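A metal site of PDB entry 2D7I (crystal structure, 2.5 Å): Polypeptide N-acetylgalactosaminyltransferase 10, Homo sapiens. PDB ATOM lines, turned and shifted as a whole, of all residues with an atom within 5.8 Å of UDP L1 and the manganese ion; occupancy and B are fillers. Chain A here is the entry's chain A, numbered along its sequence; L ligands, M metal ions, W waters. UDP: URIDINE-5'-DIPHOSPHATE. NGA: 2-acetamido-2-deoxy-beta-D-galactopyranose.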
ATOM      1  N   ILE A 118      11.594  24.851  12.859  1.00  0.00           N
ATOM      2  CA  ILE A 118      12.526  23.994  12.122  1.00  0.00           C
ATOM      3  C   ILE A 118      13.599  23.388  13.024  1.00  0.00           C
ATOM      4  O   ILE A 118      14.576  24.042  13.412  1.00  0.00           O
ATOM      5  CB  ILE A 118      13.209  24.765  10.973  1.00  0.00           C
ATOM      6  CG1 ILE A 118      12.160  25.346  10.014  1.00  0.00           C
ATOM      7  CG2 ILE A 118      14.150  23.832  10.218  1.00  0.00           C
ATOM      8  CD1 ILE A 118      12.710  26.403   9.068  1.00  0.00           C
ATOM      9  N   PRO A 119      13.421  22.112  13.392  1.00  0.00           N
ATOM     10  CA  PRO A 119      14.385  21.424  14.249  1.00  0.00           C
ATOM     11  C   PRO A 119      15.533  20.951  13.383  1.00  0.00           C
ATOM     12  O   PRO A 119      15.351  20.605  12.222  1.00  0.00           O
ATOM     13  CB  PRO A 119      13.588  20.249  14.784  1.00  0.00           C
ATOM     14  CG  PRO A 119      12.724  19.896  13.595  1.00  0.00           C
ATOM     15  CD  PRO A 119      12.248  21.253  13.131  1.00  0.00           C
ATOM     16  N   PHE A 120      16.731  20.928  13.946  1.00  0.00           N
ATOM     17  CA  PHE A 120      17.857  20.479  13.167  1.00  0.00           C
ATOM     18  C   PHE A 120      18.957  19.932  14.073  1.00  0.00           C
ATOM     19  O   PHE A 120      19.061  20.277  15.247  1.00  0.00           O
ATOM     20  CB  PHE A 120      18.373  21.624  12.291  1.00  0.00           C
ATOM     21  CG  PHE A 120      19.123  22.680  13.020  1.00  0.00           C
ATOM     22  CD1 PHE A 120      20.479  22.525  13.288  1.00  0.00           C
ATOM     23  CD2 PHE A 120      18.484  23.848  13.420  1.00  0.00           C
ATOM     24  CE1 PHE A 120      21.204  23.527  13.945  1.00  0.00           C
ATOM     25  CE2 PHE A 120      19.191  24.863  14.079  1.00  0.00           C
ATOM     26  CZ  PHE A 120      20.559  24.703  14.343  1.00  0.00           C
ATOM     27  N   HIS A 121      19.785  19.084  13.482  1.00  0.00           N
ATOM     28  CA  HIS A 121      20.880  18.460  14.200  1.00  0.00           C
ATOM     29  C   HIS A 121      21.991  18.224  13.202  1.00  0.00           C
ATOM     30  O   HIS A 121      21.835  17.443  12.261  1.00  0.00           O
ATOM     31  CB  HIS A 121      20.408  17.122  14.767  1.00  0.00           C
ATOM     32  CG  HIS A 121      21.493  16.321  15.387  1.00  0.00           C
ATOM     33  ND1 HIS A 121      22.040  16.622  16.616  1.00  0.00           N
ATOM     34  CD2 HIS A 121      22.190  15.251  14.920  1.00  0.00           C
ATOM     35  CE1 HIS A 121      23.021  15.774  16.884  1.00  0.00           C
ATOM     36  NE2 HIS A 121      23.130  14.933  15.871  1.00  0.00           N
ATOM     37  N   GLU A 123      22.930  19.697  10.738  1.00  0.00           N
ATOM     38  CA  GLU A 123      22.441  19.830   9.378  1.00  0.00           C
ATOM     39  C   GLU A 123      23.457  20.657   8.569  1.00  0.00           C
ATOM     40  O   GLU A 123      24.162  21.497   9.123  1.00  0.00           O
ATOM     41  CB  GLU A 123      21.076  20.517   9.402  1.00  0.00           C
ATOM     42  CG  GLU A 123      20.133  20.095   8.257  1.00  0.00           C
ATOM     43  CD  GLU A 123      19.862  18.598   8.263  1.00  0.00           C
ATOM     44  OE1 GLU A 123      19.329  18.071   9.272  1.00  0.00           O
ATOM     45  OE2 GLU A 123      20.199  17.948   7.248  1.00  0.00           O
ATOM     46  N   VAL A 150      15.461  25.285  15.793  1.00  0.00           N
ATOM     47  CA  VAL A 150      15.737  24.663  17.065  1.00  0.00           C
ATOM     48  C   VAL A 150      16.889  23.691  16.870  1.00  0.00           C
ATOM     49  O   VAL A 150      16.761  22.678  16.182  1.00  0.00           O
ATOM     50  CB  VAL A 150      14.488  23.927  17.606  1.00  0.00           C
ATOM     51  CG1 VAL A 150      14.697  23.499  19.081  1.00  0.00           C
ATOM     52  CG2 VAL A 150      13.274  24.844  17.485  1.00  0.00           C
ATOM     53  N   ASP A 152      19.248  20.885  17.911  1.00  0.00           N
ATOM     54  CA  ASP A 152      19.247  19.736  18.798  1.00  0.00           C
ATOM     55  C   ASP A 152      20.674  19.290  19.112  1.00  0.00           C
ATOM     56  O   ASP A 152      21.179  18.313  18.572  1.00  0.00           O
ATOM     57  CB  ASP A 152      18.456  18.564  18.201  1.00  0.00           C
ATOM     58  CG  ASP A 152      18.355  17.389  19.154  1.00  0.00           C
ATOM     59  OD1 ASP A 152      18.557  17.587  20.366  1.00  0.00           O
ATOM     60  OD2 ASP A 152      18.059  16.262  18.692  1.00  0.00           O
ATOM     61  N   ARG A 181      21.306  16.340  23.783  1.00  0.00           N
ATOM     62  CA  ARG A 181      20.621  15.704  22.658  1.00  0.00           C
ATOM     63  C   ARG A 181      19.214  15.330  23.097  1.00  0.00           C
ATOM     64  O   ARG A 181      19.046  14.527  24.008  1.00  0.00           O
ATOM     65  CB  ARG A 181      21.360  14.442  22.218  1.00  0.00           C
ATOM     66  CG  ARG A 181      20.783  13.792  20.964  1.00  0.00           C
ATOM     67  CD  ARG A 181      20.925  14.696  19.742  1.00  0.00           C
ATOM     68  NE  ARG A 181      20.491  14.030  18.515  1.00  0.00           N
ATOM     69  CZ  ARG A 181      21.124  13.005  17.935  1.00  0.00           C
ATOM     70  NH1 ARG A 181      22.237  12.514  18.464  1.00  0.00           N
ATOM     71  NH2 ARG A 181      20.631  12.466  16.840  1.00  0.00           N
ATOM     72  N   GLU A 182      18.211  15.915  22.450  1.00  0.00           N
ATOM     73  CA  GLU A 182      16.822  15.657  22.806  1.00  0.00           C
ATOM     74  C   GLU A 182      16.064  14.801  21.804  1.00  0.00           C
ATOM     75  O   GLU A 182      15.142  14.083  22.175  1.00  0.00           O
ATOM     76  CB  GLU A 182      16.091  16.990  23.012  1.00  0.00           C
ATOM     77  CG  GLU A 182      16.637  17.812  24.157  1.00  0.00           C
ATOM     78  CD  GLU A 182      16.224  17.273  25.540  1.00  0.00           C
ATOM     79  OE1 GLU A 182      16.075  16.041  25.698  1.00  0.00           O
ATOM     80  OE2 GLU A 182      16.079  18.100  26.472  1.00  0.00           O
ATOM     81  N   GLY A 183      16.451  14.870  20.526  1.00  0.00           N
ATOM     82  CA  GLY A 183      15.763  14.098  19.506  1.00  0.00           C
ATOM     83  C   GLY A 183      14.763  14.980  18.783  1.00  0.00           C
ATOM     84  O   GLY A 183      14.277  15.956  19.355  1.00  0.00           O
ATOM     85  N   LEU A 184      14.422  14.610  17.550  1.00  0.00           N
ATOM     86  CA  LEU A 184      13.505  15.419  16.766  1.00  0.00           C
ATOM     87  C   LEU A 184      12.146  15.627  17.442  1.00  0.00           C
ATOM     88  O   LEU A 184      11.606  16.739  17.436  1.00  0.00           O
ATOM     89  CB  LEU A 184      13.333  14.812  15.366  1.00  0.00           C
ATOM     90  CG  LEU A 184      12.430  13.601  15.145  1.00  0.00           C
ATOM     91  CD1 LEU A 184      10.991  14.068  14.883  1.00  0.00           C
ATOM     92  CD2 LEU A 184      12.922  12.809  13.969  1.00  0.00           C
ATOM     93  N   THR A 187      12.652  17.890  20.368  1.00  0.00           N
ATOM     94  CA  THR A 187      13.192  19.134  19.831  1.00  0.00           C
ATOM     95  C   THR A 187      12.054  19.908  19.167  1.00  0.00           C
ATOM     96  O   THR A 187      12.032  21.128  19.241  1.00  0.00           O
ATOM     97  CB  THR A 187      14.339  18.872  18.828  1.00  0.00           C
ATOM     98  OG1 THR A 187      15.395  18.152  19.491  1.00  0.00           O
ATOM     99  CG2 THR A 187      14.891  20.185  18.283  1.00  0.00           C
ATOM    100  N   ARG A 188      11.102  19.217  18.565  1.00  0.00           N
ATOM    101  CA  ARG A 188       9.977  19.927  17.947  1.00  0.00           C
ATOM    102  C   ARG A 188       9.079  20.467  19.053  1.00  0.00           C
ATOM    103  O   ARG A 188       8.470  21.521  18.906  1.00  0.00           O
ATOM    104  CB  ARG A 188       9.172  19.020  17.010  1.00  0.00           C
ATOM    105  CG  ARG A 188       9.926  18.683  15.745  1.00  0.00           C
ATOM    106  CD  ARG A 188       9.033  18.577  14.517  1.00  0.00           C
ATOM    107  NE  ARG A 188       8.378  17.281  14.425  1.00  0.00           N
ATOM    108  CZ  ARG A 188       8.518  16.456  13.390  1.00  0.00           C
ATOM    109  NH1 ARG A 188       9.283  16.792  12.373  1.00  0.00           N
ATOM    110  NH2 ARG A 188       7.886  15.282  13.389  1.00  0.00           N
ATOM    111  N   LEU A 203       8.573  22.026   9.817  1.00  0.00           N
ATOM    112  CA  LEU A 203       9.289  21.804   8.558  1.00  0.00           C
ATOM    113  C   LEU A 203      10.664  21.185   8.848  1.00  0.00           C
ATOM    114  O   LEU A 203      11.335  21.597   9.781  1.00  0.00           O
ATOM    115  CB  LEU A 203       9.501  23.146   7.879  1.00  0.00           C
ATOM    116  CG  LEU A 203       8.817  23.595   6.592  1.00  0.00           C
ATOM    117  CD1 LEU A 203       7.320  23.405   6.605  1.00  0.00           C
ATOM    118  CD2 LEU A 203       9.155  25.073   6.414  1.00  0.00           C
ATOM    119  N   ASP A 204      11.088  20.197   8.059  1.00  0.00           N
ATOM    120  CA  ASP A 204      12.411  19.633   8.280  1.00  0.00           C
ATOM    121  C   ASP A 204      13.446  20.663   7.828  1.00  0.00           C
ATOM    122  O   ASP A 204      13.122  21.582   7.081  1.00  0.00           O
ATOM    123  CB  ASP A 204      12.565  18.342   7.515  1.00  0.00           C
ATOM    124  CG  ASP A 204      12.261  17.141   8.370  1.00  0.00           C
ATOM    125  OD1 ASP A 204      11.713  17.326   9.489  1.00  0.00           O
ATOM    126  OD2 ASP A 204      12.591  16.014   7.923  1.00  0.00           O
ATOM    127  N   SER A 205      14.682  20.519   8.284  1.00  0.00           N
ATOM    128  CA  SER A 205      15.709  21.495   7.961  1.00  0.00           C
ATOM    129  C   SER A 205      16.292  21.439   6.567  1.00  0.00           C
ATOM    130  O   SER A 205      17.230  22.176   6.258  1.00  0.00           O
ATOM    131  CB  SER A 205      16.848  21.426   8.958  1.00  0.00           C
ATOM    132  OG  SER A 205      17.372  20.108   9.032  1.00  0.00           O
ATOM    133  N   HIS A 206      15.754  20.578   5.723  1.00  0.00           N
ATOM    134  CA  HIS A 206      16.238  20.443   4.350  1.00  0.00           C
ATOM    135  C   HIS A 206      15.029  20.445   3.419  1.00  0.00           C
ATOM    136  O   HIS A 206      14.754  19.457   2.745  1.00  0.00           O
ATOM    137  CB  HIS A 206      17.047  19.147   4.160  1.00  0.00           C
ATOM    138  CG  HIS A 206      16.629  18.051   5.087  1.00  0.00           C
ATOM    139  ND1 HIS A 206      17.298  17.785   6.257  1.00  0.00           N
ATOM    140  CD2 HIS A 206      15.562  17.217   5.059  1.00  0.00           C
ATOM    141  CE1 HIS A 206      16.656  16.839   6.919  1.00  0.00           C
ATOM    142  NE2 HIS A 206      15.604  16.477   6.214  1.00  0.00           N
ATOM    143  N   ILE A 308      14.805   9.497  19.425  1.00  0.00           N
ATOM    144  CA  ILE A 308      15.458  10.293  18.383  1.00  0.00           C
ATOM    145  C   ILE A 308      14.665  10.456  17.091  1.00  0.00           C
ATOM    146  O   ILE A 308      14.564  11.563  16.546  1.00  0.00           O
ATOM    147  CB  ILE A 308      16.852   9.691  18.036  1.00  0.00           C
ATOM    148  CG1 ILE A 308      17.866  10.059  19.130  1.00  0.00           C
ATOM    149  CG2 ILE A 308      17.326  10.180  16.679  1.00  0.00           C
ATOM    150  CD1 ILE A 308      17.527   9.488  20.485  1.00  0.00           C
ATOM    151  N   TRP A 309      14.091   9.364  16.611  1.00  0.00           N
ATOM    152  CA  TRP A 309      13.371   9.391  15.365  1.00  0.00           C
ATOM    153  C   TRP A 309      12.322   8.276  15.339  1.00  0.00           C
ATOM    154  O   TRP A 309      12.475   7.263  16.021  1.00  0.00           O
ATOM    155  CB  TRP A 309      14.408   9.203  14.245  1.00  0.00           C
ATOM    156  CG  TRP A 309      13.903   9.175  12.856  1.00  0.00           C
ATOM    157  CD1 TRP A 309      13.979  10.191  11.936  1.00  0.00           C
ATOM    158  CD2 TRP A 309      13.286   8.070  12.191  1.00  0.00           C
ATOM    159  NE1 TRP A 309      13.456   9.773  10.729  1.00  0.00           N
ATOM    160  CE2 TRP A 309      13.022   8.476  10.853  1.00  0.00           C
ATOM    161  CE3 TRP A 309      12.937   6.768  12.589  1.00  0.00           C
ATOM    162  CZ2 TRP A 309      12.418   7.629   9.926  1.00  0.00           C
ATOM    163  CZ3 TRP A 309      12.334   5.932  11.652  1.00  0.00           C
ATOM    164  CH2 TRP A 309      12.089   6.360  10.341  1.00  0.00           C
ATOM    165  N   HIS A 337      11.383  18.301  -0.226  1.00  0.00           N
ATOM    166  CA  HIS A 337      12.075  17.707   0.905  1.00  0.00           C
ATOM    167  C   HIS A 337      13.176  16.810   0.380  1.00  0.00           C
ATOM    168  O   HIS A 337      12.981  16.093  -0.588  1.00  0.00           O
ATOM    169  CB  HIS A 337      11.118  16.875   1.766  1.00  0.00           C
ATOM    170  CG  HIS A 337      11.788  16.128   2.865  1.00  0.00           C
ATOM    171  ND1 HIS A 337      12.268  14.846   2.713  1.00  0.00           N
ATOM    172  CD2 HIS A 337      12.132  16.496   4.128  1.00  0.00           C
ATOM    173  CE1 HIS A 337      12.871  14.462   3.822  1.00  0.00           C
ATOM    174  NE2 HIS A 337      12.799  15.451   4.696  1.00  0.00           N
ATOM    175  N   ILE A 338      14.340  16.840   1.029  1.00  0.00           N
ATOM    176  CA  ILE A 338      15.450  15.998   0.616  1.00  0.00           C
ATOM    177  C   ILE A 338      15.418  14.692   1.403  1.00  0.00           C
ATOM    178  O   ILE A 338      15.678  14.698   2.601  1.00  0.00           O
ATOM    179  CB  ILE A 338      16.807  16.674   0.926  1.00  0.00           C
ATOM    180  CG1 ILE A 338      16.871  18.070   0.312  1.00  0.00           C
ATOM    181  CG2 ILE A 338      17.960  15.801   0.402  1.00  0.00           C
ATOM    182  CD1 ILE A 338      18.178  18.779   0.602  1.00  0.00           C
ATOM    183  N   TYR A 339      15.114  13.587   0.746  1.00  0.00           N
ATOM    184  CA  TYR A 339      15.122  12.291   1.433  1.00  0.00           C
ATOM    185  C   TYR A 339      16.569  11.774   1.474  1.00  0.00           C
ATOM    186  O   TYR A 339      17.244  11.685   0.449  1.00  0.00           O
ATOM    187  CB  TYR A 339      14.224  11.284   0.712  1.00  0.00           C
ATOM    188  CG  TYR A 339      12.771  11.667   0.745  1.00  0.00           C
ATOM    189  CD1 TYR A 339      12.268  12.635  -0.122  1.00  0.00           C
ATOM    190  CD2 TYR A 339      11.911  11.094   1.674  1.00  0.00           C
ATOM    191  CE1 TYR A 339      10.945  13.022  -0.053  1.00  0.00           C
ATOM    192  CE2 TYR A 339      10.594  11.473   1.746  1.00  0.00           C
ATOM    193  CZ  TYR A 339      10.107  12.441   0.881  1.00  0.00           C
ATOM    194  OH  TYR A 339       8.793  12.853   0.967  1.00  0.00           O
ATOM    195  N   ARG A 340      17.033  11.444   2.671  1.00  0.00           N
ATOM    196  CA  ARG A 340      18.401  11.010   2.838  1.00  0.00           C
ATOM    197  C   ARG A 340      18.726   9.703   2.155  1.00  0.00           C
ATOM    198  O   ARG A 340      17.885   8.807   2.102  1.00  0.00           O
ATOM    199  CB  ARG A 340      18.736  10.868   4.320  1.00  0.00           C
ATOM    200  CG  ARG A 340      18.588  12.142   5.140  1.00  0.00           C
ATOM    201  CD  ARG A 340      18.995  11.885   6.577  1.00  0.00           C
ATOM    202  NE  ARG A 340      18.510  12.919   7.494  1.00  0.00           N
ATOM    203  CZ  ARG A 340      19.134  14.059   7.728  1.00  0.00           C
ATOM    204  NH1 ARG A 340      20.284  14.331   7.114  1.00  0.00           N
ATOM    205  NH2 ARG A 340      18.623  14.931   8.591  1.00  0.00           N
ATOM    206  N   TYR A 345      23.852  11.329  11.170  1.00  0.00           N
ATOM    207  CA  TYR A 345      24.059  11.499  12.602  1.00  0.00           C
ATOM    208  C   TYR A 345      24.108  10.199  13.382  1.00  0.00           C
ATOM    209  O   TYR A 345      23.807   9.123  12.850  1.00  0.00           O
ATOM    210  CB  TYR A 345      22.995  12.410  13.209  1.00  0.00           C
ATOM    211  CG  TYR A 345      21.566  12.100  12.849  1.00  0.00           C
ATOM    212  CD1 TYR A 345      20.917  12.797  11.823  1.00  0.00           C
ATOM    213  CD2 TYR A 345      20.813  11.154  13.563  1.00  0.00           C
ATOM    214  CE1 TYR A 345      19.573  12.579  11.518  1.00  0.00           C
ATOM    215  CE2 TYR A 345      19.462  10.923  13.275  1.00  0.00           C
ATOM    216  CZ  TYR A 345      18.854  11.637  12.249  1.00  0.00           C
ATOM    217  OH  TYR A 345      17.521  11.427  11.944  1.00  0.00           O
HETATM  218  N1  UDP L   1      16.626  16.031  13.873  1.00  0.00           N
HETATM  219  C2  UDP L   1      16.766  16.518  15.172  1.00  0.00           C
HETATM  220  N3  UDP L   1      17.247  15.699  16.156  1.00  0.00           N
HETATM  221  C4  UDP L   1      17.583  14.392  15.891  1.00  0.00           C
HETATM  222  C5  UDP L   1      17.438  13.889  14.594  1.00  0.00           C
HETATM  223  C6  UDP L   1      16.857  14.701  13.615  1.00  0.00           C
HETATM  224  O2  UDP L   1      16.488  17.682  15.455  1.00  0.00           O
HETATM  225  O4  UDP L   1      18.013  13.689  16.797  1.00  0.00           O
HETATM  226  C1' UDP L   1      16.089  16.939  12.855  1.00  0.00           C
HETATM  227  C2' UDP L   1      16.722  16.850  11.482  1.00  0.00           C
HETATM  228  O2' UDP L   1      17.797  17.760  11.362  1.00  0.00           O
HETATM  229  C3' UDP L   1      15.557  17.182  10.567  1.00  0.00           C
HETATM  230  C4' UDP L   1      14.325  16.706  11.328  1.00  0.00           C
HETATM  231  O4' UDP L   1      14.732  16.600  12.679  1.00  0.00           O
HETATM  232  O3' UDP L   1      15.420  18.582  10.388  1.00  0.00           O
HETATM  233  C5' UDP L   1      13.750  15.370  10.846  1.00  0.00           C
HETATM  234  O5' UDP L   1      14.692  14.322  10.935  1.00  0.00           O
HETATM  235  PA  UDP L   1      15.269  13.608   9.612  1.00  0.00           P
HETATM  236  O1A UDP L   1      15.326  14.550   8.466  1.00  0.00           O
HETATM  237  O2A UDP L   1      16.585  12.999   9.908  1.00  0.00           O
HETATM  238  O3A UDP L   1      14.148  12.502   9.297  1.00  0.00           O
HETATM  239  PB  UDP L   1      13.762  12.020   7.814  1.00  0.00           P
HETATM  240  O1B UDP L   1      13.088  13.098   7.041  1.00  0.00           O
HETATM  241  O2B UDP L   1      14.961  11.616   7.048  1.00  0.00           O
HETATM  242  O3B UDP L   1      12.877  10.851   8.046  1.00  0.00           O
HETATM  243  C1  NGA L   2       9.505  11.039   8.277  1.00  0.00           C
HETATM  244  C2  NGA L   2       9.545  12.562   8.362  1.00  0.00           C
HETATM  245  C3  NGA L   2      10.561  12.998   9.425  1.00  0.00           C
HETATM  246  C4  NGA L   2      10.167  12.370  10.765  1.00  0.00           C
HETATM  247  C5  NGA L   2      10.066  10.854  10.599  1.00  0.00           C
HETATM  248  C6  NGA L   2       9.581  10.242  11.918  1.00  0.00           C
HETATM  249  C7  NGA L   2       8.936  13.658   6.247  1.00  0.00           C
HETATM  250  C8  NGA L   2       9.451  14.213   4.923  1.00  0.00           C
HETATM  251  N2  NGA L   2       9.878  13.155   7.051  1.00  0.00           N
HETATM  252  O1  NGA L   2       8.536  10.652   7.303  1.00  0.00           O
HETATM  253  O3  NGA L   2      10.553  14.420   9.541  1.00  0.00           O
HETATM  254  O4  NGA L   2       8.895  12.878  11.178  1.00  0.00           O
HETATM  255  O5  NGA L   2       9.120  10.516   9.565  1.00  0.00           O
HETATM  256  O6  NGA L   2      10.477  10.591  12.980  1.00  0.00           O
HETATM  257  O7  NGA L   2       7.746  13.713   6.533  1.00  0.00           O
HETATM  258 MN    MN M   1      13.993  14.972   6.612  1.00  0.00          MN
HETATM  259  O   HOH W   1      15.437  13.948   5.543  1.00  0.00           O
HETATM  260  O   HOH W   2      14.929  10.767   4.399  1.00  0.00           O
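Three residues have an atom within 4 Å of the manganese ion: Asp 204, His 206 and His 337. The nearest printed residue that does not touch the manganese ion is Ile 338 (4.4 Å).
The manganese ion is bound by water W1 (2.1 Å), an oxygen (O1B) of UDP L1 (2.1 Å), the side-chain carboxylate (OD2) of Asp 204 (2.2 Å), a ring nitrogen (NE2) of His 206 (2.2 Å), a ring nitrogen (NE2) of His 337 (2.3 Å) and an oxygen (O1A) of UDP L1 (2.3 Å).
N of Leu 184 sits at hydrogen-bond distance from O of Ile 308. OE1 of Glu 123 lies within salt-bridge range of NH2 of Arg 340 (3.3 Å). The backbone carbonyl oxygen (O) of Val 150 is in hydrogen-bond range of the backbone NH (N) of Phe 120 (2.8 Å). OD1 of Asp 204 lies within salt-bridge range of NH1 of Arg 188 (3.8 Å). O of His 206 lies within hydrogen-bond range of N of Ile 338 (3.2 Å). The side-chain carboxylate of Asp 152 is in hydrogen-bond range of the backbone NH of Glu 182 (2.7 Å). OD2 of Asp 152 lies within hydrogen-bond range of N of Gly 183 (2.8 Å). ND1 of His 206 lies within hydrogen-bond range of OE2 of Glu 123, 3.1 Å away.
The backbone NH (N) of Leu 184 lies close to a nitrogen (N3) of UDP L1. Residues that only touch UDP L1: Phe 120 (3.3 Å), Gly 183 (3.5 Å) and Ile 308 (3.6 Å). Hydrophobic or aromatic side chains within 4 Å of UDP L1: Pro 119, His 121, Leu 184, His 206, Ile 308, Trp 309, His 337 and Tyr 345. 16 residues have an atom within 4 Å of UDP L1: Pro 119, Phe 120, His 121, Glu 123, Asp 152, Arg 181, Gly 183, Leu 184, Asp 204, Ser 205, His 206, Ile 308, Trp 309, His 337, Arg 340 and Tyr 345. Along chain A the residues within 4 Å of UDP L1 span positions 119 to 345.
OE1 of Glu 123 is in hydrogen-bond range of O2' of UDP L1, at 2.6 Å. NE of Arg 340 lies within salt-bridge range of O2A of UDP L1 (3.1 Å). The indole nitrogen (NE1) of Trp 309 is in hydrogen-bond range of an oxygen (O3B) of UDP L1. N of His 121 lies within hydrogen-bond range of O2' of UDP L1 (3.2 Å). An oxygen (O3') of UDP L1 lies within hydrogen-bond range of the backbone NH (N) of Ser 205, at 3.0 Å. O3' of UDP L1 sits at hydrogen-bond distance from O of Pro 119 (2.7 Å). The guanidinium group (NH2) of Arg 188 sits at hydrogen-bond distance from an oxygen (O4) of NGA L2 (3.4 Å). An oxygen (O3') of UDP L1 lies within hydrogen-bond range of the side-chain hydroxyl of Ser 205 (2.8 Å). NH2 of Arg 181 is in hydrogen-bond range of O4 of UDP L1, at 2.9 Å. An oxygen (O3) of NGA L2 lies within hydrogen-bond range of the side-chain carboxylate of Asp 204 (3.1 Å). The side-chain hydroxyl (OH) of Tyr 345 sits at hydrogen-bond distance from an oxygen (O2A) of UDP L1 (2.7 Å). The side-chain carboxylate (OD2) of Asp 152 sits at hydrogen-bond distance from a nitrogen (N3) of UDP L1 (2.7 Å).
Water W1 bridges O2B of UDP L1 (2.8 Å) and O of Ile 338 (3.0 Å). Water W2 lies within hydrogen-bond range of O2B of UDP L1 (2.8 Å) and N of Arg 340 (2.8 Å).
O1B of UDP L1 lies close to N2 of NGA L2.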
